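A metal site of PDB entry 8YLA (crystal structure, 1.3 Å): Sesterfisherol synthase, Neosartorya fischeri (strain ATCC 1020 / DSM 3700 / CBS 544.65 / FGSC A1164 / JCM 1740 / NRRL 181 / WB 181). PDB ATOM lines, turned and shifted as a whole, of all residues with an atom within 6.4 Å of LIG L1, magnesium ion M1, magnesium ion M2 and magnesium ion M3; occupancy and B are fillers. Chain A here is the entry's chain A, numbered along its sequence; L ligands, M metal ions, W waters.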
ATOM      1  N   ILE A  92      16.647   0.852  13.601  1.00  0.00           N
ATOM      2  CA  ILE A  92      17.595   1.976  13.617  1.00  0.00           C
ATOM      3  C   ILE A  92      18.606   1.839  12.488  1.00  0.00           C
ATOM      4  O   ILE A  92      18.895   2.803  11.783  1.00  0.00           O
ATOM      5  CB  ILE A  92      18.306   2.077  14.979  1.00  0.00           C
ATOM      6  CG1 ILE A  92      17.308   2.411  16.097  1.00  0.00           C
ATOM      7  CG2 ILE A  92      19.406   3.130  14.919  1.00  0.00           C
ATOM      8  CD1 ILE A  92      17.889   2.242  17.498  1.00  0.00           C
ATOM      9  N   ASP A  95      16.932   2.564   9.318  1.00  0.00           N
ATOM     10  CA  ASP A  95      16.597   3.987   9.211  1.00  0.00           C
ATOM     11  C   ASP A  95      17.823   4.829   8.937  1.00  0.00           C
ATOM     12  O   ASP A  95      17.730   5.834   8.215  1.00  0.00           O
ATOM     13  CB  ASP A  95      15.888   4.474  10.480  1.00  0.00           C
ATOM     14  CG  ASP A  95      15.215   5.817  10.254  1.00  0.00           C
ATOM     15  OD1 ASP A  95      14.344   5.899   9.361  1.00  0.00           O
ATOM     16  OD2 ASP A  95      15.570   6.789  10.970  1.00  0.00           O
ATOM     17  N   ASP A  96      18.970   4.430   9.474  1.00  0.00           N
ATOM     18  CA  ASP A  96      20.201   5.157   9.171  1.00  0.00           C
ATOM     19  C   ASP A  96      20.525   5.068   7.672  1.00  0.00           C
ATOM     20  O   ASP A  96      20.953   6.048   7.067  1.00  0.00           O
ATOM     21  CB  ASP A  96      21.359   4.639  10.019  1.00  0.00           C
ATOM     22  CG  ASP A  96      21.319   5.169  11.443  1.00  0.00           C
ATOM     23  OD1 ASP A  96      20.446   6.018  11.759  1.00  0.00           O
ATOM     24  OD2 ASP A  96      22.145   4.705  12.256  1.00  0.00           O
ATOM     25  N   TYR A  98      18.229   4.607   5.298  1.00  0.00           N
ATOM     26  CA  TYR A  98      17.180   5.424   4.691  1.00  0.00           C
ATOM     27  C   TYR A  98      17.548   6.901   4.702  1.00  0.00           C
ATOM     28  O   TYR A  98      17.373   7.597   3.705  1.00  0.00           O
ATOM     29  CB  TYR A  98      15.881   5.159   5.454  1.00  0.00           C
ATOM     30  CG  TYR A  98      14.745   6.125   5.248  1.00  0.00           C
ATOM     31  CD1 TYR A  98      13.807   5.910   4.243  1.00  0.00           C
ATOM     32  CD2 TYR A  98      14.571   7.209   6.102  1.00  0.00           C
ATOM     33  CE1 TYR A  98      12.745   6.774   4.072  1.00  0.00           C
ATOM     34  CE2 TYR A  98      13.504   8.080   5.925  1.00  0.00           C
ATOM     35  CZ  TYR A  98      12.590   7.848   4.914  1.00  0.00           C
ATOM     36  OH  TYR A  98      11.510   8.683   4.734  1.00  0.00           O
ATOM     37  N   GLU A  99      18.020   7.381   5.845  1.00  0.00           N
ATOM     38  CA  GLU A  99      18.368   8.795   6.000  1.00  0.00           C
ATOM     39  C   GLU A  99      19.519   9.246   5.101  1.00  0.00           C
ATOM     40  O   GLU A  99      19.631  10.420   4.774  1.00  0.00           O
ATOM     41  CB  GLU A  99      18.712   9.105   7.470  1.00  0.00           C
ATOM     42  CG  GLU A  99      17.517   9.040   8.404  1.00  0.00           C
ATOM     43  CD  GLU A  99      17.762   9.780   9.704  1.00  0.00           C
ATOM     44  OE1 GLU A  99      18.391  10.855   9.675  1.00  0.00           O
ATOM     45  OE2 GLU A  99      17.318   9.275  10.764  1.00  0.00           O
ATOM     46  N   ARG A 187       6.525  14.009  11.566  1.00  0.00           N
ATOM     47  CA  ARG A 187       7.471  13.347  12.462  1.00  0.00           C
ATOM     48  C   ARG A 187       6.848  12.113  13.100  1.00  0.00           C
ATOM     49  O   ARG A 187       7.546  11.123  13.331  1.00  0.00           O
ATOM     50  CB  ARG A 187       7.996  14.330  13.509  1.00  0.00           C
ATOM     51  CG  ARG A 187       9.022  13.739  14.431  1.00  0.00           C
ATOM     52  CD  ARG A 187      10.317  13.340  13.719  1.00  0.00           C
ATOM     53  NE  ARG A 187      11.366  13.119  14.697  1.00  0.00           N
ATOM     54  CZ  ARG A 187      12.112  12.032  14.810  1.00  0.00           C
ATOM     55  NH1 ARG A 187      12.072  11.062  13.916  1.00  0.00           N
ATOM     56  NH2 ARG A 187      12.919  11.914  15.863  1.00  0.00           N
ATOM     57  N   ASP A 190       7.581   9.559  10.557  1.00  0.00           N
ATOM     58  CA  ASP A 190       9.008   9.316  10.379  1.00  0.00           C
ATOM     59  C   ASP A 190       9.619   8.633  11.590  1.00  0.00           C
ATOM     60  O   ASP A 190      10.566   7.845  11.459  1.00  0.00           O
ATOM     61  CB  ASP A 190       9.698  10.657  10.110  1.00  0.00           C
ATOM     62  CG  ASP A 190      11.209  10.538  10.100  1.00  0.00           C
ATOM     63  OD1 ASP A 190      11.751   9.960   9.137  1.00  0.00           O
ATOM     64  OD2 ASP A 190      11.853  11.022  11.053  1.00  0.00           O
ATOM     65  N   PHE A 191       9.114   8.935  12.793  1.00  0.00           N
ATOM     66  CA  PHE A 191       9.562   8.289  14.026  1.00  0.00           C
ATOM     67  C   PHE A 191       8.975   6.898  14.186  1.00  0.00           C
ATOM     68  O   PHE A 191       9.528   6.085  14.933  1.00  0.00           O
ATOM     69  CB  PHE A 191       9.102   9.147  15.221  1.00  0.00           C
ATOM     70  CG  PHE A 191       9.622   8.705  16.558  1.00  0.00           C
ATOM     71  CD1 PHE A 191      10.816   9.220  17.055  1.00  0.00           C
ATOM     72  CD2 PHE A 191       8.890   7.832  17.368  1.00  0.00           C
ATOM     73  CE1 PHE A 191      11.286   8.851  18.309  1.00  0.00           C
ATOM     74  CE2 PHE A 191       9.368   7.452  18.620  1.00  0.00           C
ATOM     75  CZ  PHE A 191      10.555   7.967  19.089  1.00  0.00           C
ATOM     76  N   ILE A 228       9.101  11.862  21.301  1.00  0.00           N
ATOM     77  CA  ILE A 228       9.660  12.231  20.006  1.00  0.00           C
ATOM     78  C   ILE A 228      10.588  13.419  20.149  1.00  0.00           C
ATOM     79  O   ILE A 228      11.724  13.409  19.650  1.00  0.00           O
ATOM     80  CB  ILE A 228       8.526  12.490  19.010  1.00  0.00           C
ATOM     81  CG1 ILE A 228       7.766  11.196  18.744  1.00  0.00           C
ATOM     82  CG2 ILE A 228       9.071  13.101  17.738  1.00  0.00           C
ATOM     83  CD1 ILE A 228       6.535  11.378  17.901  1.00  0.00           C
ATOM     84  N   ASN A 231      14.029  12.650  21.730  1.00  0.00           N
ATOM     85  CA  ASN A 231      15.012  12.241  20.739  1.00  0.00           C
ATOM     86  C   ASN A 231      15.498  13.442  19.952  1.00  0.00           C
ATOM     87  O   ASN A 231      16.696  13.578  19.712  1.00  0.00           O
ATOM     88  CB  ASN A 231      14.487  11.171  19.795  1.00  0.00           C
ATOM     89  CG  ASN A 231      15.464  10.929  18.667  1.00  0.00           C
ATOM     90  OD1 ASN A 231      15.380  11.575  17.621  1.00  0.00           O
ATOM     91  ND2 ASN A 231      16.450  10.062  18.891  1.00  0.00           N
ATOM     92  N   ASP A 232      14.578  14.309  19.518  1.00  0.00           N
ATOM     93  CA  ASP A 232      15.014  15.444  18.685  1.00  0.00           C
ATOM     94  C   ASP A 232      16.042  16.285  19.439  1.00  0.00           C
ATOM     95  O   ASP A 232      17.068  16.682  18.873  1.00  0.00           O
ATOM     96  CB  ASP A 232      13.825  16.333  18.325  1.00  0.00           C
ATOM     97  CG  ASP A 232      12.898  15.737  17.270  1.00  0.00           C
ATOM     98  OD1 ASP A 232      13.189  14.663  16.680  1.00  0.00           O
ATOM     99  OD2 ASP A 232      11.851  16.394  17.026  1.00  0.00           O
ATOM    100  N   SER A 235      19.433  14.406  19.608  1.00  0.00           N
ATOM    101  CA  SER A 235      20.010  14.019  18.324  1.00  0.00           C
ATOM    102  C   SER A 235      20.222  15.194  17.373  1.00  0.00           C
ATOM    103  O   SER A 235      20.717  14.984  16.265  1.00  0.00           O
ATOM    104  CB  SER A 235      19.209  12.891  17.652  1.00  0.00           C
ATOM    105  OG  SER A 235      17.873  13.267  17.338  1.00  0.00           O
ATOM    106  N   PHE A 236      19.906  16.417  17.794  1.00  0.00           N
ATOM    107  CA  PHE A 236      20.034  17.566  16.898  1.00  0.00           C
ATOM    108  C   PHE A 236      21.458  17.720  16.362  1.00  0.00           C
ATOM    109  O   PHE A 236      21.652  17.923  15.157  1.00  0.00           O
ATOM    110  CB  PHE A 236      19.592  18.862  17.571  1.00  0.00           C
ATOM    111  CG  PHE A 236      19.859  20.079  16.723  1.00  0.00           C
ATOM    112  CD1 PHE A 236      18.971  20.472  15.736  1.00  0.00           C
ATOM    113  CD2 PHE A 236      21.022  20.835  16.891  1.00  0.00           C
ATOM    114  CE1 PHE A 236      19.218  21.579  14.938  1.00  0.00           C
ATOM    115  CE2 PHE A 236      21.283  21.942  16.097  1.00  0.00           C
ATOM    116  CZ  PHE A 236      20.377  22.328  15.121  1.00  0.00           C
ATOM    117  N   ARG A 238      23.982  15.721  15.761  1.00  0.00           N
ATOM    118  CA  ARG A 238      24.333  14.763  14.707  1.00  0.00           C
ATOM    119  C   ARG A 238      23.526  15.035  13.450  1.00  0.00           C
ATOM    120  O   ARG A 238      24.068  15.029  12.337  1.00  0.00           O
ATOM    121  CB  ARG A 238      24.093  13.331  15.181  1.00  0.00           C
ATOM    122  CG  ARG A 238      24.032  12.297  14.032  1.00  0.00           C
ATOM    123  CD  ARG A 238      24.037  10.872  14.531  1.00  0.00           C
ATOM    124  NE  ARG A 238      23.060  10.641  15.584  1.00  0.00           N
ATOM    125  CZ  ARG A 238      21.740  10.522  15.409  1.00  0.00           C
ATOM    126  NH1 ARG A 238      21.185  10.652  14.213  1.00  0.00           N
ATOM    127  NH2 ARG A 238      20.978  10.279  16.465  1.00  0.00           N
ATOM    128  N   GLU A 239      22.228  15.236  13.600  1.00  0.00           N
ATOM    129  CA  GLU A 239      21.360  15.403  12.452  1.00  0.00           C
ATOM    130  C   GLU A 239      21.668  16.697  11.703  1.00  0.00           C
ATOM    131  O   GLU A 239      21.633  16.720  10.464  1.00  0.00           O
ATOM    132  CB  GLU A 239      19.893  15.329  12.903  1.00  0.00           C
ATOM    133  CG  GLU A 239      19.558  13.935  13.368  1.00  0.00           C
ATOM    134  CD  GLU A 239      18.232  13.825  14.086  1.00  0.00           C
ATOM    135  OE1 GLU A 239      17.541  14.869  14.229  1.00  0.00           O
ATOM    136  OE2 GLU A 239      17.896  12.679  14.484  1.00  0.00           O
ATOM    137  N   THR A 251      15.167  16.437  10.164  1.00  0.00           N
ATOM    138  CA  THR A 251      13.819  16.217  10.698  1.00  0.00           C
ATOM    139  C   THR A 251      13.947  16.324  12.219  1.00  0.00           C
ATOM    140  O   THR A 251      14.228  15.347  12.906  1.00  0.00           O
ATOM    141  CB  THR A 251      13.275  14.860  10.268  1.00  0.00           C
ATOM    142  OG1 THR A 251      13.443  14.714   8.849  1.00  0.00           O
ATOM    143  CG2 THR A 251      11.810  14.756  10.625  1.00  0.00           C
ATOM    144  N   ASN A 252      13.736  17.528  12.754  1.00  0.00           N
ATOM    145  CA  ASN A 252      14.047  17.761  14.153  1.00  0.00           C
ATOM    146  C   ASN A 252      13.337  19.025  14.617  1.00  0.00           C
ATOM    147  O   ASN A 252      13.476  20.072  13.981  1.00  0.00           O
ATOM    148  CB  ASN A 252      15.575  17.886  14.303  1.00  0.00           C
ATOM    149  CG  ASN A 252      16.009  17.852  15.736  1.00  0.00           C
ATOM    150  OD1 ASN A 252      15.578  18.686  16.533  1.00  0.00           O
ATOM    151  ND2 ASN A 252      16.853  16.907  16.086  1.00  0.00           N
ATOM    152  N   TRP A 318      19.044   7.609  28.575  1.00  0.00           N
ATOM    153  CA  TRP A 318      19.957   6.973  27.638  1.00  0.00           C
ATOM    154  C   TRP A 318      20.504   7.978  26.630  1.00  0.00           C
ATOM    155  O   TRP A 318      21.701   8.022  26.355  1.00  0.00           O
ATOM    156  CB  TRP A 318      19.241   5.824  26.933  1.00  0.00           C
ATOM    157  CG  TRP A 318      20.115   5.071  25.993  1.00  0.00           C
ATOM    158  CD1 TRP A 318      20.887   3.991  26.302  1.00  0.00           C
ATOM    159  CD2 TRP A 318      20.344   5.338  24.598  1.00  0.00           C
ATOM    160  NE1 TRP A 318      21.583   3.567  25.188  1.00  0.00           N
ATOM    161  CE2 TRP A 318      21.267   4.380  24.134  1.00  0.00           C
ATOM    162  CE3 TRP A 318      19.849   6.296  23.699  1.00  0.00           C
ATOM    163  CZ2 TRP A 318      21.694   4.341  22.800  1.00  0.00           C
ATOM    164  CZ3 TRP A 318      20.285   6.245  22.363  1.00  0.00           C
ATOM    165  CH2 TRP A 318      21.195   5.282  21.938  1.00  0.00           C
ATOM    166  N   ARG A 324      25.594   7.323  20.132  1.00  0.00           N
ATOM    167  CA  ARG A 324      24.969   7.652  18.855  1.00  0.00           C
ATOM    168  C   ARG A 324      24.732   9.147  18.690  1.00  0.00           C
ATOM    169  O   ARG A 324      25.063   9.724  17.654  1.00  0.00           O
ATOM    170  CB  ARG A 324      23.652   6.887  18.708  1.00  0.00           C
ATOM    171  CG  ARG A 324      22.861   7.240  17.460  1.00  0.00           C
ATOM    172  CD  ARG A 324      21.657   6.322  17.296  1.00  0.00           C
ATOM    173  NE  ARG A 324      20.845   6.699  16.141  1.00  0.00           N
ATOM    174  CZ  ARG A 324      20.940   6.131  14.944  1.00  0.00           C
ATOM    175  NH1 ARG A 324      21.823   5.167  14.728  1.00  0.00           N
ATOM    176  NH2 ARG A 324      20.156   6.538  13.956  1.00  0.00           N
ATOM    177  N   HIS A 325      24.401   9.754  19.830  1.00  0.00           N
ATOM    178  CA  HIS A 325      24.077  11.189  19.808  1.00  0.00           C
ATOM    179  C   HIS A 325      25.187  12.140  20.173  1.00  0.00           C
ATOM    180  O   HIS A 325      25.213  13.248  19.866  1.00  0.00           O
ATOM    181  CB  HIS A 325      22.887  11.505  20.758  1.00  0.00           C
ATOM    182  CG  HIS A 325      21.656  10.701  20.527  1.00  0.00           C
ATOM    183  ND1 HIS A 325      21.235  10.292  19.284  1.00  0.00           N
ATOM    184  CD2 HIS A 325      20.720  10.280  21.399  1.00  0.00           C
ATOM    185  CE1 HIS A 325      20.107   9.631  19.419  1.00  0.00           C
ATOM    186  NE2 HIS A 325      19.755   9.620  20.686  1.00  0.00           N
HETATM  187  O1  LIG L   1      13.975   9.005  14.592  1.00  0.00           O
HETATM  188  P1  LIG L   1      15.395   9.449  14.394  1.00  0.00           P
HETATM  189  O2  LIG L   1      15.587  10.916  14.662  1.00  0.00           O
HETATM  190  O3  LIG L   1      15.926   9.037  13.048  1.00  0.00           O
HETATM  191  O4  LIG L   1      16.295   8.652  15.476  1.00  0.00           O
HETATM  192  P2  LIG L   1      17.852   8.992  15.799  1.00  0.00           P
HETATM  193  O5  LIG L   1      18.314   7.976  16.808  1.00  0.00           O
HETATM  194  O6  LIG L   1      18.594   8.881  14.483  1.00  0.00           O
HETATM  195  O7  LIG L   1      17.923  10.389  16.363  1.00  0.00           O
HETATM  196  N1  LG2 L   2      13.198   4.342  15.262  1.00  0.00           N
HETATM  197  C1  LG2 L   2      13.296   2.884  15.393  1.00  0.00           C
HETATM  198  C2  LG2 L   2      13.017   4.701  13.843  1.00  0.00           C
HETATM  199  C3  LG2 L   2      11.558   4.571  13.474  1.00  0.00           C
HETATM  200  C4  LG2 L   2      12.062   4.838  16.047  1.00  0.00           C
HETATM  201  C5  LG2 L   2      12.347   4.644  17.521  1.00  0.00           C
HETATM  202  C6  LG2 L   2      14.447   4.951  15.760  1.00  0.00           C
HETATM  203  C7  LG2 L   2      14.193   6.412  16.077  1.00  0.00           C
HETATM  204  C8  LG2 L   2      11.904   2.284  15.420  1.00  0.00           C
HETATM  205  C9  LG2 L   2      11.226   2.177  16.623  1.00  0.00           C
HETATM  206  C10 LG2 L   2       9.948   1.616  16.660  1.00  0.00           C
HETATM  207  C11 LG2 L   2       9.361   1.173  15.477  1.00  0.00           C
HETATM  208  C12 LG2 L   2      10.040   1.280  14.274  1.00  0.00           C
HETATM  209  C13 LG2 L   2      11.315   1.830  14.244  1.00  0.00           C
HETATM  210 MG    MG M   1      16.698  11.987  15.983  1.00  0.00          MG
HETATM  211 MG    MG M   2      15.078   8.774  11.168  1.00  0.00          MG
HETATM  212 MG    MG M   3      18.004   8.938  12.556  1.00  0.00          MG
HETATM  213  O   HOH W   1      14.468  10.784  10.986  1.00  0.00           O
HETATM  214  O   HOH W   2      14.191   8.661   9.280  1.00  0.00           O
HETATM  215  O   HOH W   3      13.298   8.225  12.121  1.00  0.00           O
HETATM  216  O   HOH W   4      15.540  13.691  15.637  1.00  0.00           O
HETATM  217  O   HOH W   5      18.399  10.953  12.477  1.00  0.00           O
HETATM  218  O   HOH W   6      17.847   6.870  12.330  1.00  0.00           O
HETATM  219  O   HOH W   7      19.869   8.710  11.664  1.00  0.00           O
HETATM  220  O   HOH W   8      15.360  12.767  12.563  1.00  0.00           O
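The guanidinium group (NH2) of Arg 238 lies within salt-bridge range of an oxygen (O5) of LIG L1 (3.5 Å). An oxygen (O5) of LIG L1 lies within salt-bridge range of the guanidinium group of Arg 324 (2.9 Å). The guanidinium group of Arg 187 lies within salt-bridge range of an oxygen (O1) of LIG L1, at 2.9 Å.
The side-chain carboxylate of Asp 96 lies within salt-bridge range of the guanidinium group of Arg 324. The backbone carbonyl oxygen (O) of Arg 324 sits at hydrogen-bond distance from the guanidinium group (NE) of Arg 238 (3.0 Å). The guanidinium group (NH1) of Arg 187 lies within salt-bridge range of the side-chain carboxylate (OD2) of Asp 190 (2.9 Å). A ring nitrogen (ND1) of His 325 is in hydrogen-bond range of the guanidinium group (NH2) of Arg 238 (2.8 Å). OE2 of Glu 239 sits close to NH1 of Arg 238 (3.9 Å). OD1 of Asn 231 sits close to NH2 of Arg 187 (3.0 Å). OD1 of Asp 232 is in salt-bridge range of NH2 of Arg 187, 2.9 Å away. ND2 of Asn 252 is in hydrogen-bond range of OE1 of Glu 239 (2.8 Å).
His 325 touches LIG L1 (CE1 to O5, 3.6 Å). Of the 20 residues printed, 9 come within 4 Å of LIG L1. The nearest printed residue that does not touch LIG L1 is Phe 191 (4.01 Å).
Residues that only touch magnesium ion M1: Arg 187. Of the 20 residues printed, 4 come within 4 Å of magnesium ion M1. The nearest printed residue that does not touch magnesium ion M1 is Asp 232 (4.5 Å).
Asp 190 touches magnesium ion M2 (OD2 to MG, 3.9 Å).
Asp 96 touches magnesium ion M3. Arg 238 touches magnesium ion M3. Arg 324 touches magnesium ion M3 (NH2 to MG, 3.5 Å). Within 4 Å of magnesium ion M3: Asp 95, Asp 96, Glu 99, Arg 238 and Arg 324.
Magnesium ion M1 is bound by an oxygen (O2) of LIG L1 (2.0 Å), the side-chain carboxylate of Glu 239 (2.0 Å), an oxygen (O7) of LIG L1 (2.0 Å), water W4 (2.1 Å), the side-chain amide oxygen of Asn 231 (2.1 Å) and the side-chain hydroxyl of Ser 235 (2.2 Å). Magnesium ion M1 has six donor atoms within binding distance.
OD2 of Asp 95 binds magnesium ion M2 (2.1 Å). O3 of LIG L1 is bound to magnesium ion M2 (2.1 Å). Water W2 is bound to magnesium ion M2. Magnesium ion M2 is bound by water W3 (2.1 Å). Water W1 is bound to magnesium ion M2 (2.1 Å). Magnesium ion M2 is bound by OE2 of Glu 99 (2.3 Å). Magnesium ion M2 has six donor atoms within binding distance.
OE2 of Glu 99 binds magnesium ion M3, 1.9 Å away. Magnesium ion M3 is bound by O6 of LIG L1. Magnesium ion M3 is bound by water W5, at 2.1 Å. Water W7 binds magnesium ion M3 (2.1 Å). Water W6 is bound to magnesium ion M3 (2.1 Å). O3 of LIG L1 binds magnesium ion M3 (2.1 Å).
Water W2 bridges OD1 of Asp 95 (2.8 Å) and OD1 of Asp 190 (2.8 Å). Water W3 lies within hydrogen-bond range of O1 of LIG L1 (2.7 Å) and O of Asp 190 (2.8 Å). Water W6 lies within hydrogen-bond range of the side-chain carboxylate of Asp 96 (2.8 Å) and the guanidinium group of Arg 324 (2.8 Å). Water W7 lies within hydrogen-bond range of OD1 of Asp 96 (2.8 Å), NH2 of Arg 324 (3.2 Å), OE1 of Glu 99 (3.3 Å) and NH1 of Arg 238 (3.5 Å). Water W5 lies within hydrogen-bond range of the side-chain carboxylate (OE1) of Glu 99 (2.8 Å) and the guanidinium group (NH1) of Arg 238 (3.3 Å). Water W8 bridges O of Thr 251 and OE1 of Glu 239.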
